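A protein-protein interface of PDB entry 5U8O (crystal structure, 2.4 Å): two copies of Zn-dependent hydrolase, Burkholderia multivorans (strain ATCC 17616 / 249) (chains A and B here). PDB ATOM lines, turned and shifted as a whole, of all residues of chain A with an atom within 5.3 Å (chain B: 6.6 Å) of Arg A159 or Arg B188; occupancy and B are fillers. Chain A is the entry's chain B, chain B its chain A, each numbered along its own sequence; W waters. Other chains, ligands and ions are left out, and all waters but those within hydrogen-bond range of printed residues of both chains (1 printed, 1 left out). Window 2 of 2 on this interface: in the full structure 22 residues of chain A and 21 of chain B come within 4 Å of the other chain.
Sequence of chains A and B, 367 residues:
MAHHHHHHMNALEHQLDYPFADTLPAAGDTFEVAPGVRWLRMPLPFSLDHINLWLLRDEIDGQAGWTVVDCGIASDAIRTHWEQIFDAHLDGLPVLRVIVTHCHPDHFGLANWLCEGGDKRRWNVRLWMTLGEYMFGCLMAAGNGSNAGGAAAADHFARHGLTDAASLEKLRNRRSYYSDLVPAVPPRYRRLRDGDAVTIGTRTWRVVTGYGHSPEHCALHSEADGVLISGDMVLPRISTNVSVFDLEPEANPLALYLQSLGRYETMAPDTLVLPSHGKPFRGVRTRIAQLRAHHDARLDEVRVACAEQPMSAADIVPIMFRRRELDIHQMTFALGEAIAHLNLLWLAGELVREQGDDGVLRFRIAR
N of Tyr B189 lies within hydrogen-bond range of O of Leu A247 (3.1 Å).
The backbone carbonyl oxygen (O) of Pro B186 lies within hydrogen-bond range of the side-chain hydroxyl (OH) of Tyr B134. OD2 of Asp A155 is in salt-bridge range of NH2 of Arg A159, 2.7 Å away. O of Arg A159 sits at hydrogen-bond distance from N of Leu A361.
NH1 of Arg A159 touches NH2 of Arg B188, 3.9 Å away. Arg B188 touches Asp A246 (CG to O, 3.5 Å). Leu A247 touches Tyr B134 (CD1 to OH, 3.5 Å). CD1 of Leu A247 touches O of Pro B187 (3.6 Å). CA of Arg B188 touches O of Leu A247 (3.3 Å). CG of Pro A249 touches NH2 of Arg B126 (3.8 Å). Pro A249 touches Arg B188.
Ala A154 touches none of the printed residues of chain B. Of chain B, only Arg B188 (3.9 Å) comes within 4 Å of Arg A159. Of the printed residues of chain B, Asp A246 touches Arg B188 (3.5 Å). Of the printed residues of chain B, Leu A247 touches Tyr B134 (3.5 Å), Pro B187 (3.6 Å), Arg B188 (3.3 Å) and Tyr B189 (3.1 Å). Of the printed residues of chain A, Arg B126 touches Pro A249 (3.8 Å). Of the printed residues of chain A, Arg B188 touches Arg A159, Asp A246, Leu A247 and Pro A249. Of the printed residues of chain A, Tyr B189 touches Leu A247 (3.1 Å). The nearest printed residue of chain B that does not touch Arg A159 is Arg B126 (8.3 Å). The nearest residue of chain A that does not touch Arg B188 is Asp A155 (4.5 Å). The nearest printed residue of chain B that does not touch Pro A249 is Tyr B189 (4.02 Å).
Of the 14 printed residues of chain A, 4 touch a printed residue of chain B.
No position is printed for both chains. Of the 8 pairs that touch across the chains among the printed residues, none has its exchanged pair printed and touching as well.
Water W1 lies within hydrogen-bond range of O of Asp A246 (2.8 Å) and NE of Arg B188 (3.0 Å).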
ATOM      1  N   ALA A 154      10.066 -20.199  17.795  1.00  0.00           N
ATOM      2  CA  ALA A 154       8.843 -19.438  18.048  1.00  0.00           C
ATOM      3  C   ALA A 154       9.006 -18.515  19.244  1.00  0.00           C
ATOM      4  O   ALA A 154       8.485 -17.395  19.238  1.00  0.00           O
ATOM      5  CB  ALA A 154       7.656 -20.381  18.265  1.00  0.00           C
ATOM      6  N   ASP A 155       9.707 -18.973  20.289  1.00  0.00           N
ATOM      7  CA  ASP A 155       9.970 -18.110  21.436  1.00  0.00           C
ATOM      8  C   ASP A 155      10.926 -16.974  21.061  1.00  0.00           C
ATOM      9  O   ASP A 155      10.712 -15.823  21.460  1.00  0.00           O
ATOM     10  CB  ASP A 155      10.524 -18.950  22.592  1.00  0.00           C
ATOM     11  CG  ASP A 155      10.526 -18.210  23.925  1.00  0.00           C
ATOM     12  OD1 ASP A 155       9.446 -17.984  24.530  1.00  0.00           O
ATOM     13  OD2 ASP A 155      11.636 -17.868  24.377  1.00  0.00           O
ATOM     14  N   HIS A 156      11.938 -17.262  20.233  1.00  0.00           N
ATOM     15  CA  HIS A 156      12.854 -16.222  19.759  1.00  0.00           C
ATOM     16  C   HIS A 156      12.116 -15.137  18.983  1.00  0.00           C
ATOM     17  O   HIS A 156      12.262 -13.944  19.279  1.00  0.00           O
ATOM     18  CB  HIS A 156      13.939 -16.847  18.887  1.00  0.00           C
ATOM     19  CG  HIS A 156      14.840 -15.857  18.215  1.00  0.00           C
ATOM     20  ND1 HIS A 156      15.705 -15.039  18.917  1.00  0.00           N
ATOM     21  CD2 HIS A 156      15.049 -15.591  16.902  1.00  0.00           C
ATOM     22  CE1 HIS A 156      16.389 -14.297  18.063  1.00  0.00           C
ATOM     23  NE2 HIS A 156      16.013 -14.614  16.836  1.00  0.00           N
ATOM     24  N   PHE A 157      11.321 -15.528  17.978  1.00  0.00           N
ATOM     25  CA  PHE A 157      10.606 -14.528  17.192  1.00  0.00           C
ATOM     26  C   PHE A 157       9.483 -13.866  17.985  1.00  0.00           C
ATOM     27  O   PHE A 157       9.141 -12.710  17.719  1.00  0.00           O
ATOM     28  CB  PHE A 157      10.104 -15.149  15.889  1.00  0.00           C
ATOM     29  CG  PHE A 157      11.221 -15.470  14.921  1.00  0.00           C
ATOM     30  CD1 PHE A 157      12.074 -14.463  14.479  1.00  0.00           C
ATOM     31  CD2 PHE A 157      11.436 -16.764  14.476  1.00  0.00           C
ATOM     32  CE1 PHE A 157      13.118 -14.740  13.600  1.00  0.00           C
ATOM     33  CE2 PHE A 157      12.473 -17.052  13.599  1.00  0.00           C
ATOM     34  CZ  PHE A 157      13.312 -16.040  13.156  1.00  0.00           C
ATOM     35  N   ALA A 158       8.917 -14.558  18.971  1.00  0.00           N
ATOM     36  CA  ALA A 158       7.920 -13.918  19.831  1.00  0.00           C
ATOM     37  C   ALA A 158       8.511 -12.750  20.611  1.00  0.00           C
ATOM     38  O   ALA A 158       7.873 -11.700  20.725  1.00  0.00           O
ATOM     39  CB  ALA A 158       7.307 -14.926  20.803  1.00  0.00           C
ATOM     40  N   ARG A 159       9.717 -12.908  21.172  1.00  0.00           N
ATOM     41  CA  ARG A 159      10.307 -11.762  21.870  1.00  0.00           C
ATOM     42  C   ARG A 159      10.809 -10.691  20.916  1.00  0.00           C
ATOM     43  O   ARG A 159      11.124  -9.587  21.361  1.00  0.00           O
ATOM     44  CB  ARG A 159      11.415 -12.168  22.851  1.00  0.00           C
ATOM     45  CG  ARG A 159      12.679 -12.710  22.279  1.00  0.00           C
ATOM     46  CD  ARG A 159      13.689 -12.910  23.409  1.00  0.00           C
ATOM     47  NE  ARG A 159      13.101 -13.673  24.501  1.00  0.00           N
ATOM     48  CZ  ARG A 159      13.056 -15.000  24.550  1.00  0.00           C
ATOM     49  NH1 ARG A 159      13.558 -15.723  23.548  1.00  0.00           N
ATOM     50  NH2 ARG A 159      12.482 -15.600  25.591  1.00  0.00           N
ATOM     51  N   HIS A 160      10.870 -10.968  19.620  1.00  0.00           N
ATOM     52  CA  HIS A 160      11.196  -9.929  18.659  1.00  0.00           C
ATOM     53  C   HIS A 160       9.959  -9.427  17.933  1.00  0.00           C
ATOM     54  O   HIS A 160      10.066  -8.864  16.839  1.00  0.00           O
ATOM     55  CB  HIS A 160      12.268 -10.410  17.695  1.00  0.00           C
ATOM     56  CG  HIS A 160      13.634 -10.403  18.305  1.00  0.00           C
ATOM     57  ND1 HIS A 160      14.389  -9.258  18.407  1.00  0.00           N
ATOM     58  CD2 HIS A 160      14.358 -11.381  18.895  1.00  0.00           C
ATOM     59  CE1 HIS A 160      15.535  -9.533  19.001  1.00  0.00           C
ATOM     60  NE2 HIS A 160      15.542 -10.817  19.305  1.00  0.00           N
ATOM     61  N   GLY A 161       8.785  -9.635  18.516  1.00  0.00           N
ATOM     62  CA  GLY A 161       7.589  -8.932  18.101  1.00  0.00           C
ATOM     63  C   GLY A 161       6.546  -9.752  17.380  1.00  0.00           C
ATOM     64  O   GLY A 161       5.445  -9.241  17.173  1.00  0.00           O
ATOM     65  N   ASP A 246      17.867 -18.143  17.301  1.00  0.00           N
ATOM     66  CA  ASP A 246      17.740 -18.345  18.743  1.00  0.00           C
ATOM     67  C   ASP A 246      19.033 -18.825  19.396  1.00  0.00           C
ATOM     68  O   ASP A 246      19.251 -18.566  20.588  1.00  0.00           O
ATOM     69  CB  ASP A 246      16.621 -19.349  19.036  1.00  0.00           C
ATOM     70  CG  ASP A 246      16.921 -20.749  18.478  1.00  0.00           C
ATOM     71  OD1 ASP A 246      16.749 -20.962  17.251  1.00  0.00           O
ATOM     72  OD2 ASP A 246      17.359 -21.626  19.257  1.00  0.00           O
ATOM     73  N   LEU A 247      19.867 -19.558  18.652  1.00  0.00           N
ATOM     74  CA  LEU A 247      21.071 -20.168  19.215  1.00  0.00           C
ATOM     75  C   LEU A 247      22.093 -19.114  19.616  1.00  0.00           C
ATOM     76  O   LEU A 247      22.816 -19.272  20.610  1.00  0.00           O
ATOM     77  CB  LEU A 247      21.690 -21.119  18.195  1.00  0.00           C
ATOM     78  CG  LEU A 247      22.692 -22.134  18.710  1.00  0.00           C
ATOM     79  CD1 LEU A 247      21.984 -23.082  19.672  1.00  0.00           C
ATOM     80  CD2 LEU A 247      23.338 -22.899  17.563  1.00  0.00           C
ATOM     81  N   PRO A 249      21.589 -15.347  20.036  1.00  0.00           N
ATOM     82  CA  PRO A 249      20.655 -14.214  19.950  1.00  0.00           C
ATOM     83  C   PRO A 249      21.322 -12.849  19.937  1.00  0.00           C
ATOM     84  O   PRO A 249      20.688 -11.882  19.493  1.00  0.00           O
ATOM     85  CB  PRO A 249      19.768 -14.396  21.192  1.00  0.00           C
ATOM     86  CG  PRO A 249      20.631 -15.157  22.165  1.00  0.00           C
ATOM     87  CD  PRO A 249      21.470 -16.078  21.311  1.00  0.00           C
ATOM     88  N   GLY A 359       7.352  -8.767  27.260  1.00  0.00           N
ATOM     89  CA  GLY A 359       8.431  -9.660  26.913  1.00  0.00           C
ATOM     90  C   GLY A 359       9.105  -9.370  25.588  1.00  0.00           C
ATOM     91  O   GLY A 359      10.050 -10.083  25.232  1.00  0.00           O
ATOM     92  N   VAL A 360       8.718  -8.293  24.887  1.00  0.00           N
ATOM     93  CA  VAL A 360       9.260  -8.000  23.564  1.00  0.00           C
ATOM     94  C   VAL A 360      10.461  -7.077  23.695  1.00  0.00           C
ATOM     95  O   VAL A 360      10.450  -6.116  24.476  1.00  0.00           O
ATOM     96  CB  VAL A 360       8.196  -7.370  22.644  1.00  0.00           C
ATOM     97  CG1 VAL A 360       8.848  -6.937  21.293  1.00  0.00           C
ATOM     98  CG2 VAL A 360       7.024  -8.330  22.430  1.00  0.00           C
ATOM     99  N   LEU A 361      11.509  -7.388  22.929  1.00  0.00           N
ATOM    100  CA  LEU A 361      12.694  -6.554  22.859  1.00  0.00           C
ATOM    101  C   LEU A 361      12.449  -5.419  21.875  1.00  0.00           C
ATOM    102  O   LEU A 361      11.985  -5.642  20.748  1.00  0.00           O
ATOM    103  CB  LEU A 361      13.909  -7.389  22.430  1.00  0.00           C
ATOM    104  CG  LEU A 361      14.385  -8.453  23.427  1.00  0.00           C
ATOM    105  CD1 LEU A 361      15.220  -9.544  22.749  1.00  0.00           C
ATOM    106  CD2 LEU A 361      15.173  -7.806  24.588  1.00  0.00           C
ATOM    107  N   CYS B 115      25.911 -21.169  34.255  1.00  0.00           N
ATOM    108  CA  CYS B 115      25.052 -20.198  33.589  1.00  0.00           C
ATOM    109  C   CYS B 115      23.687 -20.108  34.257  1.00  0.00           C
ATOM    110  O   CYS B 115      23.072 -19.035  34.265  1.00  0.00           O
ATOM    111  CB  CYS B 115      24.912 -20.558  32.108  1.00  0.00           C
ATOM    112  SG  CYS B 115      26.402 -20.216  31.133  1.00  0.00           S
ATOM    113  N   ARG B 126      25.210 -15.561  30.306  1.00  0.00           N
ATOM    114  CA  ARG B 126      25.439 -16.066  28.956  1.00  0.00           C
ATOM    115  C   ARG B 126      26.771 -16.807  28.855  1.00  0.00           C
ATOM    116  O   ARG B 126      27.781 -16.365  29.404  1.00  0.00           O
ATOM    117  CB  ARG B 126      25.413 -14.911  27.931  1.00  0.00           C
ATOM    118  CG  ARG B 126      25.907 -15.273  26.489  1.00  0.00           C
ATOM    119  CD  ARG B 126      24.885 -16.109  25.731  1.00  0.00           C
ATOM    120  NE  ARG B 126      23.658 -15.359  25.476  1.00  0.00           N
ATOM    121  CZ  ARG B 126      22.533 -15.492  26.175  1.00  0.00           C
ATOM    122  NH1 ARG B 126      22.487 -16.354  27.187  1.00  0.00           N
ATOM    123  NH2 ARG B 126      21.459 -14.761  25.860  1.00  0.00           N
ATOM    124  N   LEU B 127      26.760 -17.933  28.133  1.00  0.00           N
ATOM    125  CA  LEU B 127      27.972 -18.643  27.741  1.00  0.00           C
ATOM    126  C   LEU B 127      28.640 -17.964  26.545  1.00  0.00           C
ATOM    127  O   LEU B 127      27.968 -17.603  25.576  1.00  0.00           O
ATOM    128  CB  LEU B 127      27.638 -20.087  27.377  1.00  0.00           C
ATOM    129  CG  LEU B 127      28.795 -20.858  26.724  1.00  0.00           C
ATOM    130  CD1 LEU B 127      29.786 -21.338  27.782  1.00  0.00           C
ATOM    131  CD2 LEU B 127      28.285 -22.023  25.880  1.00  0.00           C
ATOM    132  N   TRP B 128      29.959 -17.768  26.630  1.00  0.00           N
ATOM    133  CA  TRP B 128      30.782 -17.252  25.538  1.00  0.00           C
ATOM    134  C   TRP B 128      31.719 -18.359  25.048  1.00  0.00           C
ATOM    135  O   TRP B 128      32.448 -18.956  25.849  1.00  0.00           O
ATOM    136  CB  TRP B 128      31.593 -16.019  25.985  1.00  0.00           C
ATOM    137  CG  TRP B 128      30.787 -14.773  26.275  1.00  0.00           C
ATOM    138  CD1 TRP B 128      29.714 -14.661  27.123  1.00  0.00           C
ATOM    139  CD2 TRP B 128      31.009 -13.461  25.746  1.00  0.00           C
ATOM    140  NE1 TRP B 128      29.241 -13.366  27.130  1.00  0.00           N
ATOM    141  CE2 TRP B 128      30.021 -12.609  26.299  1.00  0.00           C
ATOM    142  CE3 TRP B 128      31.943 -12.920  24.864  1.00  0.00           C
ATOM    143  CZ2 TRP B 128      29.939 -11.252  25.984  1.00  0.00           C
ATOM    144  CZ3 TRP B 128      31.871 -11.559  24.567  1.00  0.00           C
ATOM    145  CH2 TRP B 128      30.865 -10.749  25.113  1.00  0.00           C
ATOM    146  N   TYR B 134      31.459 -24.841  20.451  1.00  0.00           N
ATOM    147  CA  TYR B 134      30.084 -24.967  20.924  1.00  0.00           C
ATOM    148  C   TYR B 134      29.307 -26.013  20.116  1.00  0.00           C
ATOM    149  O   TYR B 134      28.587 -26.839  20.690  1.00  0.00           O
ATOM    150  CB  TYR B 134      29.386 -23.614  20.877  1.00  0.00           C
ATOM    151  CG  TYR B 134      27.928 -23.688  21.292  1.00  0.00           C
ATOM    152  CD1 TYR B 134      27.576 -23.878  22.626  1.00  0.00           C
ATOM    153  CD2 TYR B 134      26.905 -23.582  20.346  1.00  0.00           C
ATOM    154  CE1 TYR B 134      26.249 -23.939  23.012  1.00  0.00           C
ATOM    155  CE2 TYR B 134      25.580 -23.648  20.718  1.00  0.00           C
ATOM    156  CZ  TYR B 134      25.258 -23.828  22.057  1.00  0.00           C
ATOM    157  OH  TYR B 134      23.943 -23.895  22.434  1.00  0.00           O
ATOM    158  N   VAL B 185      23.958 -28.643  28.270  1.00  0.00           N
ATOM    159  CA  VAL B 185      24.697 -27.658  27.493  1.00  0.00           C
ATOM    160  C   VAL B 185      23.839 -26.400  27.491  1.00  0.00           C
ATOM    161  O   VAL B 185      22.610 -26.507  27.468  1.00  0.00           O
ATOM    162  CB  VAL B 185      24.987 -28.194  26.084  1.00  0.00           C
ATOM    163  CG1 VAL B 185      25.298 -27.068  25.129  1.00  0.00           C
ATOM    164  CG2 VAL B 185      26.123 -29.188  26.142  1.00  0.00           C
ATOM    165  N   PRO B 186      24.405 -25.203  27.599  1.00  0.00           N
ATOM    166  CA  PRO B 186      23.571 -24.014  27.524  1.00  0.00           C
ATOM    167  C   PRO B 186      22.894 -23.945  26.169  1.00  0.00           C
ATOM    168  O   PRO B 186      23.500 -24.278  25.134  1.00  0.00           O
ATOM    169  CB  PRO B 186      24.561 -22.861  27.717  1.00  0.00           C
ATOM    170  CG  PRO B 186      25.731 -23.464  28.399  1.00  0.00           C
ATOM    171  CD  PRO B 186      25.812 -24.873  27.867  1.00  0.00           C
ATOM    172  N   PRO B 187      21.618 -23.560  26.140  1.00  0.00           N
ATOM    173  CA  PRO B 187      20.882 -23.524  24.873  1.00  0.00           C
ATOM    174  C   PRO B 187      21.208 -22.310  24.017  1.00  0.00           C
ATOM    175  O   PRO B 187      20.724 -22.216  22.888  1.00  0.00           O
ATOM    176  CB  PRO B 187      19.411 -23.505  25.333  1.00  0.00           C
ATOM    177  CG  PRO B 187      19.462 -22.829  26.672  1.00  0.00           C
ATOM    178  CD  PRO B 187      20.766 -23.255  27.303  1.00  0.00           C
ATOM    179  N   ARG B 188      22.024 -21.387  24.513  1.00  0.00           N
ATOM    180  CA  ARG B 188      22.441 -20.224  23.752  1.00  0.00           C
ATOM    181  C   ARG B 188      23.890 -19.952  24.077  1.00  0.00           C
ATOM    182  O   ARG B 188      24.403 -20.359  25.122  1.00  0.00           O
ATOM    183  CB  ARG B 188      21.620 -18.983  24.099  1.00  0.00           C
ATOM    184  CG  ARG B 188      20.135 -19.168  23.951  1.00  0.00           C
ATOM    185  CD  ARG B 188      19.447 -18.016  24.621  1.00  0.00           C
ATOM    186  NE  ARG B 188      18.025 -18.257  24.766  1.00  0.00           N
ATOM    187  CZ  ARG B 188      17.269 -17.649  25.668  1.00  0.00           C
ATOM    188  NH1 ARG B 188      17.823 -16.786  26.514  1.00  0.00           N
ATOM    189  NH2 ARG B 188      15.971 -17.922  25.740  1.00  0.00           N
ATOM    190  N   TYR B 189      24.540 -19.224  23.182  1.00  0.00           N
ATOM    191  CA  TYR B 189      25.904 -18.823  23.413  1.00  0.00           C
ATOM    192  C   TYR B 189      26.110 -17.518  22.675  1.00  0.00           C
ATOM    193  O   TYR B 189      25.312 -17.144  21.800  1.00  0.00           O
ATOM    194  CB  TYR B 189      26.902 -19.900  22.957  1.00  0.00           C
ATOM    195  CG  TYR B 189      27.250 -19.910  21.475  1.00  0.00           C
ATOM    196  CD1 TYR B 189      26.272 -20.140  20.511  1.00  0.00           C
ATOM    197  CD2 TYR B 189      28.565 -19.722  21.044  1.00  0.00           C
ATOM    198  CE1 TYR B 189      26.586 -20.163  19.164  1.00  0.00           C
ATOM    199  CE2 TYR B 189      28.902 -19.756  19.700  1.00  0.00           C
ATOM    200  CZ  TYR B 189      27.904 -19.971  18.764  1.00  0.00           C
ATOM    201  OH  TYR B 189      28.210 -19.997  17.421  1.00  0.00           O
ATOM    202  N   ARG B 190      27.162 -16.808  23.088  1.00  0.00           N
ATOM    203  CA  ARG B 190      27.674 -15.632  22.406  1.00  0.00           C
ATOM    204  C   ARG B 190      29.011 -16.017  21.791  1.00  0.00           C
ATOM    205  O   ARG B 190      29.922 -16.465  22.503  1.00  0.00           O
ATOM    206  CB  ARG B 190      27.826 -14.446  23.361  1.00  0.00           C
ATOM    207  CG  ARG B 190      28.438 -13.201  22.718  1.00  0.00           C
ATOM    208  CD  ARG B 190      27.760 -11.948  23.223  1.00  0.00           C
ATOM    209  NE  ARG B 190      28.346 -10.738  22.654  1.00  0.00           N
ATOM    210  CZ  ARG B 190      27.983  -9.509  22.998  1.00  0.00           C
ATOM    211  NH1 ARG B 190      27.033  -9.334  23.909  1.00  0.00           N
ATOM    212  NH2 ARG B 190      28.575  -8.460  22.439  1.00  0.00           N
HETATM  213  O   HOH W   1      17.067 -17.506  22.037  1.00  0.00           O
